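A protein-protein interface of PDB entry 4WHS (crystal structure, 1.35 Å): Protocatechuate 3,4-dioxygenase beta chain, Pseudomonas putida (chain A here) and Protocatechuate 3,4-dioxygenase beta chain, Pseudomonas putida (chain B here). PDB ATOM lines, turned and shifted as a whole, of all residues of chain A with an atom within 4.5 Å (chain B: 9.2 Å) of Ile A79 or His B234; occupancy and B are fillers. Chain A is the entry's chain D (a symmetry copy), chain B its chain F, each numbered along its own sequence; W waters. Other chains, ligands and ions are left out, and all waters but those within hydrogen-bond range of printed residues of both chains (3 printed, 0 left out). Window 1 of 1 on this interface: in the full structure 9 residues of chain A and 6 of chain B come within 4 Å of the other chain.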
ATOM      1  N   ILE A  78       7.997  -2.141  -0.085  1.00  0.00           N
ATOM      2  CA  ILE A  78       8.271  -2.095   1.364  1.00  0.00           C
ATOM      3  C   ILE A  78       9.432  -2.987   1.742  1.00  0.00           C
ATOM      4  O   ILE A  78       9.615  -4.085   1.208  1.00  0.00           O
ATOM      5  CB  ILE A  78       7.058  -2.484   2.248  1.00  0.00           C
ATOM      6  CG1 ILE A  78       6.510  -3.874   1.912  1.00  0.00           C
ATOM      7  CG2 ILE A  78       5.962  -1.428   2.159  1.00  0.00           C
ATOM      8  CD1 ILE A  78       5.501  -4.412   2.914  1.00  0.00           C
ATOM      9  N   ILE A  79      10.200  -2.510   2.708  1.00  0.00           N
ATOM     10  CA  ILE A  79      11.128  -3.351   3.449  1.00  0.00           C
ATOM     11  C   ILE A  79      10.401  -3.895   4.678  1.00  0.00           C
ATOM     12  O   ILE A  79       9.636  -3.161   5.320  1.00  0.00           O
ATOM     13  CB  ILE A  79      12.370  -2.530   3.860  1.00  0.00           C
ATOM     14  CG1 ILE A  79      13.172  -2.168   2.597  1.00  0.00           C
ATOM     15  CG2 ILE A  79      13.216  -3.257   4.898  1.00  0.00           C
ATOM     16  CD1 ILE A  79      14.176  -1.074   2.821  1.00  0.00           C
ATOM     17  N   VAL A  80      10.588  -5.179   4.966  1.00  0.00           N
ATOM     18  CA  VAL A  80      10.068  -5.787   6.194  1.00  0.00           C
ATOM     19  C   VAL A  80      11.286  -6.288   6.951  1.00  0.00           C
ATOM     20  O   VAL A  80      12.026  -7.139   6.465  1.00  0.00           O
ATOM     21  CB  VAL A  80       9.085  -6.938   5.925  1.00  0.00           C
ATOM     22  CG1 VAL A  80       8.598  -7.565   7.220  1.00  0.00           C
ATOM     23  CG2 VAL A  80       7.912  -6.447   5.082  1.00  0.00           C
ATOM     24  N   ALA A  81      11.533  -5.709   8.117  1.00  0.00           N
ATOM     25  CA  ALA A  81      12.737  -5.994   8.878  1.00  0.00           C
ATOM     26  C   ALA A  81      12.408  -6.068  10.351  1.00  0.00           C
ATOM     27  O   ALA A  81      11.369  -5.594  10.798  1.00  0.00           O
ATOM     28  CB  ALA A  81      13.769  -4.912   8.641  1.00  0.00           C
ATOM     29  N   SER A 138      16.066  -8.919   7.229  1.00  0.00           N
ATOM     30  CA  SER A 138      15.492  -7.936   6.311  1.00  0.00           C
ATOM     31  C   SER A 138      15.040  -8.573   5.003  1.00  0.00           C
ATOM     32  O   SER A 138      15.777  -9.371   4.389  1.00  0.00           O
ATOM     33  CB  SER A 138      16.507  -6.835   6.024  1.00  0.00           C
ATOM     34  OG  SER A 138      15.925  -5.799   5.271  1.00  0.00           O
ATOM     35  N   PHE A 139      13.822  -8.237   4.602  1.00  0.00           N
ATOM     36  CA  PHE A 139      13.253  -8.602   3.310  1.00  0.00           C
ATOM     37  C   PHE A 139      12.838  -7.343   2.573  1.00  0.00           C
ATOM     38  O   PHE A 139      12.539  -6.321   3.198  1.00  0.00           O
ATOM     39  CB  PHE A 139      11.981  -9.436   3.470  1.00  0.00           C
ATOM     40  CG  PHE A 139      12.193 -10.763   4.118  1.00  0.00           C
ATOM     41  CD1 PHE A 139      12.734 -11.820   3.403  1.00  0.00           C
ATOM     42  CD2 PHE A 139      11.829 -10.979   5.435  1.00  0.00           C
ATOM     43  CE1 PHE A 139      12.937 -13.044   4.001  1.00  0.00           C
ATOM     44  CE2 PHE A 139      12.009 -12.211   6.025  1.00  0.00           C
ATOM     45  CZ  PHE A 139      12.545 -13.257   5.302  1.00  0.00           C
ATOM     46  N   ARG A 140      12.770  -7.419   1.243  1.00  0.00           N
ATOM     47  CA  ARG A 140      12.111  -6.375   0.462  1.00  0.00           C
ATOM     48  C   ARG A 140      11.001  -7.034  -0.344  1.00  0.00           C
ATOM     49  O   ARG A 140      11.188  -8.121  -0.878  1.00  0.00           O
ATOM     50  CB  ARG A 140      13.097  -5.654  -0.459  1.00  0.00           C
ATOM     51  CG  ARG A 140      12.469  -4.455  -1.165  1.00  0.00           C
ATOM     52  CD  ARG A 140      13.473  -3.617  -1.936  1.00  0.00           C
ATOM     53  NE  ARG A 140      14.057  -4.344  -3.057  1.00  0.00           N
ATOM     54  CZ  ARG A 140      14.666  -3.772  -4.087  1.00  0.00           C
ATOM     55  NH1 ARG A 140      15.163  -4.523  -5.067  1.00  0.00           N
ATOM     56  NH2 ARG A 140      14.788  -2.453  -4.161  1.00  0.00           N
ATOM     57  N   ASN A 212      13.536   3.452   8.483  1.00  0.00           N
ATOM     58  CA  ASN A 212      14.144   2.411   7.654  1.00  0.00           C
ATOM     59  C   ASN A 212      13.735   2.502   6.182  1.00  0.00           C
ATOM     60  O   ASN A 212      14.180   1.692   5.361  1.00  0.00           O
ATOM     61  CB  ASN A 212      13.757   1.041   8.205  1.00  0.00           C
ATOM     62  CG  ASN A 212      14.918   0.111   8.325  1.00  0.00           C
ATOM     63  OD1 ASN A 212      16.066   0.541   8.462  1.00  0.00           O
ATOM     64  ND2 ASN A 212      14.639  -1.180   8.234  1.00  0.00           N
ATOM     65  N   ASN A 214      13.493   3.960   2.324  1.00  0.00           N
ATOM     66  CA  ASN A 214      14.347   4.586   1.326  1.00  0.00           C
ATOM     67  C   ASN A 214      13.523   5.660   0.630  1.00  0.00           C
ATOM     68  O   ASN A 214      12.586   5.336  -0.111  1.00  0.00           O
ATOM     69  CB  ASN A 214      14.836   3.573   0.273  1.00  0.00           C
ATOM     70  CG  ASN A 214      15.968   2.679   0.755  1.00  0.00           C
ATOM     71  OD1 ASN A 214      16.559   2.887   1.802  1.00  0.00           O
ATOM     72  ND2 ASN A 214      16.272   1.668  -0.038  1.00  0.00           N
ATOM     73  N   CYS A 218      10.952   3.180  -1.333  1.00  0.00           N
ATOM     74  CA  CYS A 218      10.149   2.199  -0.613  1.00  0.00           C
ATOM     75  C   CYS A 218       9.942   2.594   0.831  1.00  0.00           C
ATOM     76  O   CYS A 218      10.790   3.223   1.451  1.00  0.00           O
ATOM     77  CB  CYS A 218      10.790   0.810  -0.663  1.00  0.00           C
ATOM     78  SG  CYS A 218      12.392   0.624   0.180  1.00  0.00           S
ATOM     79  N   LEU A 219       8.795   2.190   1.362  1.00  0.00           N
ATOM     80  CA  LEU A 219       8.504   2.337   2.781  1.00  0.00           C
ATOM     81  C   LEU A 219       9.083   1.132   3.533  1.00  0.00           C
ATOM     82  O   LEU A 219       9.816   0.326   2.956  1.00  0.00           O
ATOM     83  CB  LEU A 219       6.999   2.534   3.000  1.00  0.00           C
ATOM     84  CG  LEU A 219       6.552   3.966   2.727  1.00  0.00           C
ATOM     85  CD1 LEU A 219       5.035   4.053   2.658  1.00  0.00           C
ATOM     86  CD2 LEU A 219       7.076   4.925   3.784  1.00  0.00           C
ATOM     87  N   ALA A 220       8.833   1.054   4.838  1.00  0.00           N
ATOM     88  CA  ALA A 220       9.353  -0.011   5.663  1.00  0.00           C
ATOM     89  C   ALA A 220       8.410  -0.271   6.830  1.00  0.00           C
ATOM     90  O   ALA A 220       7.768   0.655   7.332  1.00  0.00           O
ATOM     91  CB  ALA A 220      10.744   0.346   6.179  1.00  0.00           C
ATOM     92  N   TYR A 221       8.388  -1.526   7.266  1.00  0.00           N
ATOM     93  CA  TYR A 221       7.659  -2.001   8.426  1.00  0.00           C
ATOM     94  C   TYR A 221       8.618  -2.796   9.299  1.00  0.00           C
ATOM     95  O   TYR A 221       9.550  -3.452   8.790  1.00  0.00           O
ATOM     96  CB  TYR A 221       6.469  -2.886   8.004  1.00  0.00           C
ATOM     97  CG  TYR A 221       5.311  -2.046   7.577  1.00  0.00           C
ATOM     98  CD1 TYR A 221       5.198  -1.562   6.278  1.00  0.00           C
ATOM     99  CD2 TYR A 221       4.326  -1.680   8.493  1.00  0.00           C
ATOM    100  CE1 TYR A 221       4.160  -0.705   5.918  1.00  0.00           C
ATOM    101  CE2 TYR A 221       3.282  -0.859   8.152  1.00  0.00           C
ATOM    102  CZ  TYR A 221       3.193  -0.370   6.869  1.00  0.00           C
ATOM    103  OH  TYR A 221       2.142   0.466   6.555  1.00  0.00           O
ATOM    104  N   ASN B   5      28.879   5.050   3.643  1.00  0.00           N
ATOM    105  CA  ASN B   5      28.415   3.729   4.075  1.00  0.00           C
ATOM    106  C   ASN B   5      27.186   3.768   4.959  1.00  0.00           C
ATOM    107  O   ASN B   5      26.710   2.733   5.414  1.00  0.00           O
ATOM    108  CB  ASN B   5      29.544   2.945   4.756  1.00  0.00           C
ATOM    109  CG  ASN B   5      30.317   3.772   5.761  1.00  0.00           C
ATOM    110  OD1 ASN B   5      29.731   4.419   6.630  1.00  0.00           O
ATOM    111  ND2 ASN B   5      31.647   3.752   5.651  1.00  0.00           N
ATOM    112  N   SER B   6      26.642   4.949   5.180  1.00  0.00           N
ATOM    113  CA  SER B   6      25.543   5.056   6.124  1.00  0.00           C
ATOM    114  C   SER B   6      24.566   6.142   5.709  1.00  0.00           C
ATOM    115  O   SER B   6      24.868   7.008   4.858  1.00  0.00           O
ATOM    116  CB  SER B   6      26.056   5.323   7.540  1.00  0.00           C
ATOM    117  OG  SER B   6      26.651   6.589   7.588  1.00  0.00           O
ATOM    118  N   ARG B   7      23.383   6.043   6.305  1.00  0.00           N
ATOM    119  CA  ARG B   7      22.318   7.007   6.147  1.00  0.00           C
ATOM    120  C   ARG B   7      21.932   7.512   7.522  1.00  0.00           C
ATOM    121  O   ARG B   7      22.035   6.795   8.503  1.00  0.00           O
ATOM    122  CB  ARG B   7      21.104   6.368   5.446  1.00  0.00           C
ATOM    123  CG  ARG B   7      21.377   5.895   4.023  1.00  0.00           C
ATOM    124  CD  ARG B   7      21.487   7.051   3.050  1.00  0.00           C
ATOM    125  NE  ARG B   7      21.993   6.652   1.740  1.00  0.00           N
ATOM    126  CZ  ARG B   7      23.248   6.783   1.330  1.00  0.00           C
ATOM    127  NH1 ARG B   7      24.194   7.258   2.116  1.00  0.00           N
ATOM    128  NH2 ARG B   7      23.561   6.405   0.096  1.00  0.00           N
ATOM    129  N   TYR B  88      19.195   5.645  17.678  1.00  0.00           N
ATOM    130  CA  TYR B  88      19.075   4.199  17.924  1.00  0.00           C
ATOM    131  C   TYR B  88      19.675   3.793  19.277  1.00  0.00           C
ATOM    132  O   TYR B  88      19.639   2.619  19.650  1.00  0.00           O
ATOM    133  CB  TYR B  88      19.768   3.400  16.814  1.00  0.00           C
ATOM    134  CG  TYR B  88      19.151   3.596  15.435  1.00  0.00           C
ATOM    135  CD1 TYR B  88      17.950   2.988  15.093  1.00  0.00           C
ATOM    136  CD2 TYR B  88      19.787   4.373  14.468  1.00  0.00           C
ATOM    137  CE1 TYR B  88      17.390   3.146  13.830  1.00  0.00           C
ATOM    138  CE2 TYR B  88      19.237   4.543  13.206  1.00  0.00           C
ATOM    139  CZ  TYR B  88      18.044   3.935  12.887  1.00  0.00           C
ATOM    140  OH  TYR B  88      17.506   4.119  11.633  1.00  0.00           O
ATOM    141  N   ARG B 231      22.251   4.478  10.182  1.00  0.00           N
ATOM    142  CA  ARG B 231      22.023   3.098   9.751  1.00  0.00           C
ATOM    143  C   ARG B 231      22.815   2.802   8.499  1.00  0.00           C
ATOM    144  O   ARG B 231      23.185   3.688   7.745  1.00  0.00           O
ATOM    145  CB  ARG B 231      20.540   2.801   9.506  1.00  0.00           C
ATOM    146  CG  ARG B 231      19.905   3.537   8.332  1.00  0.00           C
ATOM    147  CD  ARG B 231      18.561   2.928   8.000  1.00  0.00           C
ATOM    148  NE  ARG B 231      17.809   3.621   6.949  1.00  0.00           N
ATOM    149  CZ  ARG B 231      18.054   3.512   5.638  1.00  0.00           C
ATOM    150  NH1 ARG B 231      19.087   2.811   5.189  1.00  0.00           N
ATOM    151  NH2 ARG B 231      17.277   4.150   4.776  1.00  0.00           N
ATOM    152  N   LYS B 232      23.040   1.518   8.267  1.00  0.00           N
ATOM    153  CA  LYS B 232      23.639   1.073   7.018  1.00  0.00           C
ATOM    154  C   LYS B 232      22.678   1.337   5.864  1.00  0.00           C
ATOM    155  O   LYS B 232      21.472   1.308   6.033  1.00  0.00           O
ATOM    156  CB  LYS B 232      23.967  -0.427   7.093  1.00  0.00           C
ATOM    157  CG  LYS B 232      25.108  -0.768   8.030  1.00  0.00           C
ATOM    158  CD  LYS B 232      25.495  -2.235   7.932  1.00  0.00           C
ATOM    159  CE  LYS B 232      26.699  -2.540   8.810  1.00  0.00           C
ATOM    160  NZ  LYS B 232      27.198  -3.935   8.617  1.00  0.00           N
ATOM    161  N   THR B 233      23.223   1.625   4.695  1.00  0.00           N
ATOM    162  CA  THR B 233      22.434   1.642   3.471  1.00  0.00           C
ATOM    163  C   THR B 233      21.843   0.252   3.212  1.00  0.00           C
ATOM    164  O   THR B 233      22.427  -0.764   3.593  1.00  0.00           O
ATOM    165  CB  THR B 233      23.298   2.044   2.267  1.00  0.00           C
ATOM    166  OG1 THR B 233      24.349   1.092   2.095  1.00  0.00           O
ATOM    167  CG2 THR B 233      23.880   3.431   2.467  1.00  0.00           C
ATOM    168  N   HIS B 234      20.679   0.213   2.573  1.00  0.00           N
ATOM    169  CA  HIS B 234      20.083  -1.048   2.157  1.00  0.00           C
ATOM    170  C   HIS B 234      19.240  -0.876   0.912  1.00  0.00           C
ATOM    171  O   HIS B 234      18.572   0.145   0.736  1.00  0.00           O
ATOM    172  CB  HIS B 234      19.281  -1.728   3.278  1.00  0.00           C
ATOM    173  CG  HIS B 234      18.292  -0.855   4.003  1.00  0.00           C
ATOM    174  ND1 HIS B 234      17.436   0.045   3.399  1.00  0.00           N
ATOM    175  CD2 HIS B 234      17.996  -0.818   5.324  1.00  0.00           C
ATOM    176  CE1 HIS B 234      16.680   0.616   4.324  1.00  0.00           C
ATOM    177  NE2 HIS B 234      16.998   0.105   5.494  1.00  0.00           N
ATOM    178  N   PHE B 235      19.284  -1.891   0.055  1.00  0.00           N
ATOM    179  CA  PHE B 235      18.463  -1.962  -1.157  1.00  0.00           C
ATOM    180  C   PHE B 235      18.536  -0.701  -2.025  1.00  0.00           C
ATOM    181  O   PHE B 235      17.536  -0.292  -2.605  1.00  0.00           O
ATOM    182  CB  PHE B 235      17.003  -2.264  -0.781  1.00  0.00           C
ATOM    183  CG  PHE B 235      16.819  -3.546  -0.017  1.00  0.00           C
ATOM    184  CD1 PHE B 235      16.865  -4.777  -0.655  1.00  0.00           C
ATOM    185  CD2 PHE B 235      16.535  -3.519   1.337  1.00  0.00           C
ATOM    186  CE1 PHE B 235      16.676  -5.957   0.056  1.00  0.00           C
ATOM    187  CE2 PHE B 235      16.344  -4.688   2.049  1.00  0.00           C
ATOM    188  CZ  PHE B 235      16.409  -5.908   1.411  1.00  0.00           C
ATOM    189  N   GLU B 236      19.713  -0.074  -2.110  1.00  0.00           N
ATOM    190  CA  GLU B 236      19.864   1.103  -2.979  1.00  0.00           C
ATOM    191  C   GLU B 236      20.355   0.726  -4.379  1.00  0.00           C
ATOM    192  O   GLU B 236      21.074  -0.257  -4.549  1.00  0.00           O
ATOM    193  CB  GLU B 236      20.758   2.165  -2.335  1.00  0.00           C
ATOM    194  CG  GLU B 236      20.121   2.791  -1.103  1.00  0.00           C
ATOM    195  CD  GLU B 236      20.802   4.060  -0.620  1.00  0.00           C
ATOM    196  OE1 GLU B 236      21.738   4.583  -1.283  1.00  0.00           O
ATOM    197  OE2 GLU B 236      20.373   4.542   0.445  1.00  0.00           O
ATOM    198  N   ASN B 237      19.941   1.516  -5.370  1.00  0.00           N
ATOM    199  CA  ASN B 237      20.310   1.312  -6.787  1.00  0.00           C
ATOM    200  C   ASN B 237      19.894  -0.044  -7.357  1.00  0.00           C
ATOM    201  O   ASN B 237      20.566  -0.587  -8.241  1.00  0.00           O
ATOM    202  CB  ASN B 237      21.814   1.546  -6.997  1.00  0.00           C
ATOM    203  CG  ASN B 237      22.261   2.912  -6.515  1.00  0.00           C
ATOM    204  OD1 ASN B 237      21.573   3.910  -6.739  1.00  0.00           O
ATOM    205  ND2 ASN B 237      23.414   2.973  -5.853  1.00  0.00           N
ATOM    206  N   CYS B 238      18.788  -0.586  -6.856  1.00  0.00           N
ATOM    207  CA  CYS B 238      18.273  -1.875  -7.314  1.00  0.00           C
ATOM    208  C   CYS B 238      16.776  -1.955  -7.049  1.00  0.00           C
ATOM    209  O   CYS B 238      16.137  -2.966  -7.321  1.00  0.00           O
ATOM    210  CB  CYS B 238      19.001  -3.033  -6.619  1.00  0.00           C
ATOM    211  SG  CYS B 238      18.721  -3.163  -4.833  1.00  0.00           S
HETATM  212  O   HOH W   1      14.691  -0.298  -2.333  1.00  0.00           O
HETATM  213  O   HOH W   2      16.164   1.874  10.978  1.00  0.00           O
HETATM  214  O   HOH W   3      19.302   2.794   2.328  1.00  0.00           O
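Ile A78 touches none of the printed residues of chain B. Of the printed residues of chain B, Asn A212 touches Arg B231 (3.5 Å) and His B234 (2.9 Å). No residue of chain B comes within 4 Å of Ala A220. Ser B6 touches none of the printed residues of chain A. Lys B232 touches none of the printed residues of chain A. His B234 touches just these residues of chain A: Ile A79, Asn A212 and Asn A214. Printed residues of chain A within 4 Å of Phe B235: Ile A79 (3.7 Å), Ser A138 (3.4 Å), Arg A140 (3.6 Å) and Asn A214 (3.5 Å). The nearest residue of chain B that does not touch Ile A79 is Arg B231 (6.4 Å). The nearest printed residue of chain A that does not touch His B234 is Ser A138 (5.4 Å). The nearest printed residue of chain A that does not touch Phe B235 is Phe A139 (4.02 Å).
The backbone carbonyl oxygen of Phe B235 is in hydrogen-bond range of the side-chain amide nitrogen of Asn A214, 3.5 Å away. The guanidinium group (NH2) of Arg B231 sits at hydrogen-bond distance from the side-chain amide oxygen (OD1) of Asn A214. ND2 of Asn A214 is in hydrogen-bond range of O of His B234. A ring nitrogen (NE2) of His B234 sits at hydrogen-bond distance from the side-chain amide oxygen (OD1) of Asn A212 (3.1 Å). The backbone carbonyl oxygen of Cys B238 sits at hydrogen-bond distance from the guanidinium group of Arg A140 (2.9 Å).
The backbone carbonyl oxygen of Ile A79 lies within hydrogen-bond range of the backbone NH of Tyr A221 (2.8 Å). The backbone NH of Ile A79 is in hydrogen-bond range of the backbone carbonyl oxygen of Leu A219. The guanidinium group (NH1) of Arg B231 sits close to a ring nitrogen (NE2) of His B234, 3.4 Å away. O of Glu B236 sits at hydrogen-bond distance from SG of Cys B238 (3.7 Å). N of Arg B7 is in hydrogen-bond range of O of Arg B231 (2.8 Å).
CD1 of Ile A79 touches CE1 of His B234, at 3.4 Å. Ile A79 touches Phe B235 (CD1 to CD2, 3.7 Å). CE2 of Phe B235 touches OG of Ser A138, 3.4 Å away. CB of Arg A140 touches CE1 of Phe B235, at 3.6 Å. Arg B231 touches Asn A212.
Hydrophobic or aromatic side chains of chain A that line the printed part of chain B: Ile A79.
Water W2 bridges the side-chain hydroxyl of Tyr B88 (2.7 Å) and the side-chain amide oxygen of Asn A212 (2.8 Å). Water W3 lies within hydrogen-bond range of the side-chain carboxylate of Glu B236, the side-chain amide oxygen of Asn A214, the guanidinium group of Arg B231 and the backbone NH of His B234. Water W1 lies within hydrogen-bond range of the guanidinium group of Arg A140, the backbone carbonyl oxygen of Phe B235, the side-chain amide nitrogen of Asn A214 and the side-chain sulfur of Cys A218.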
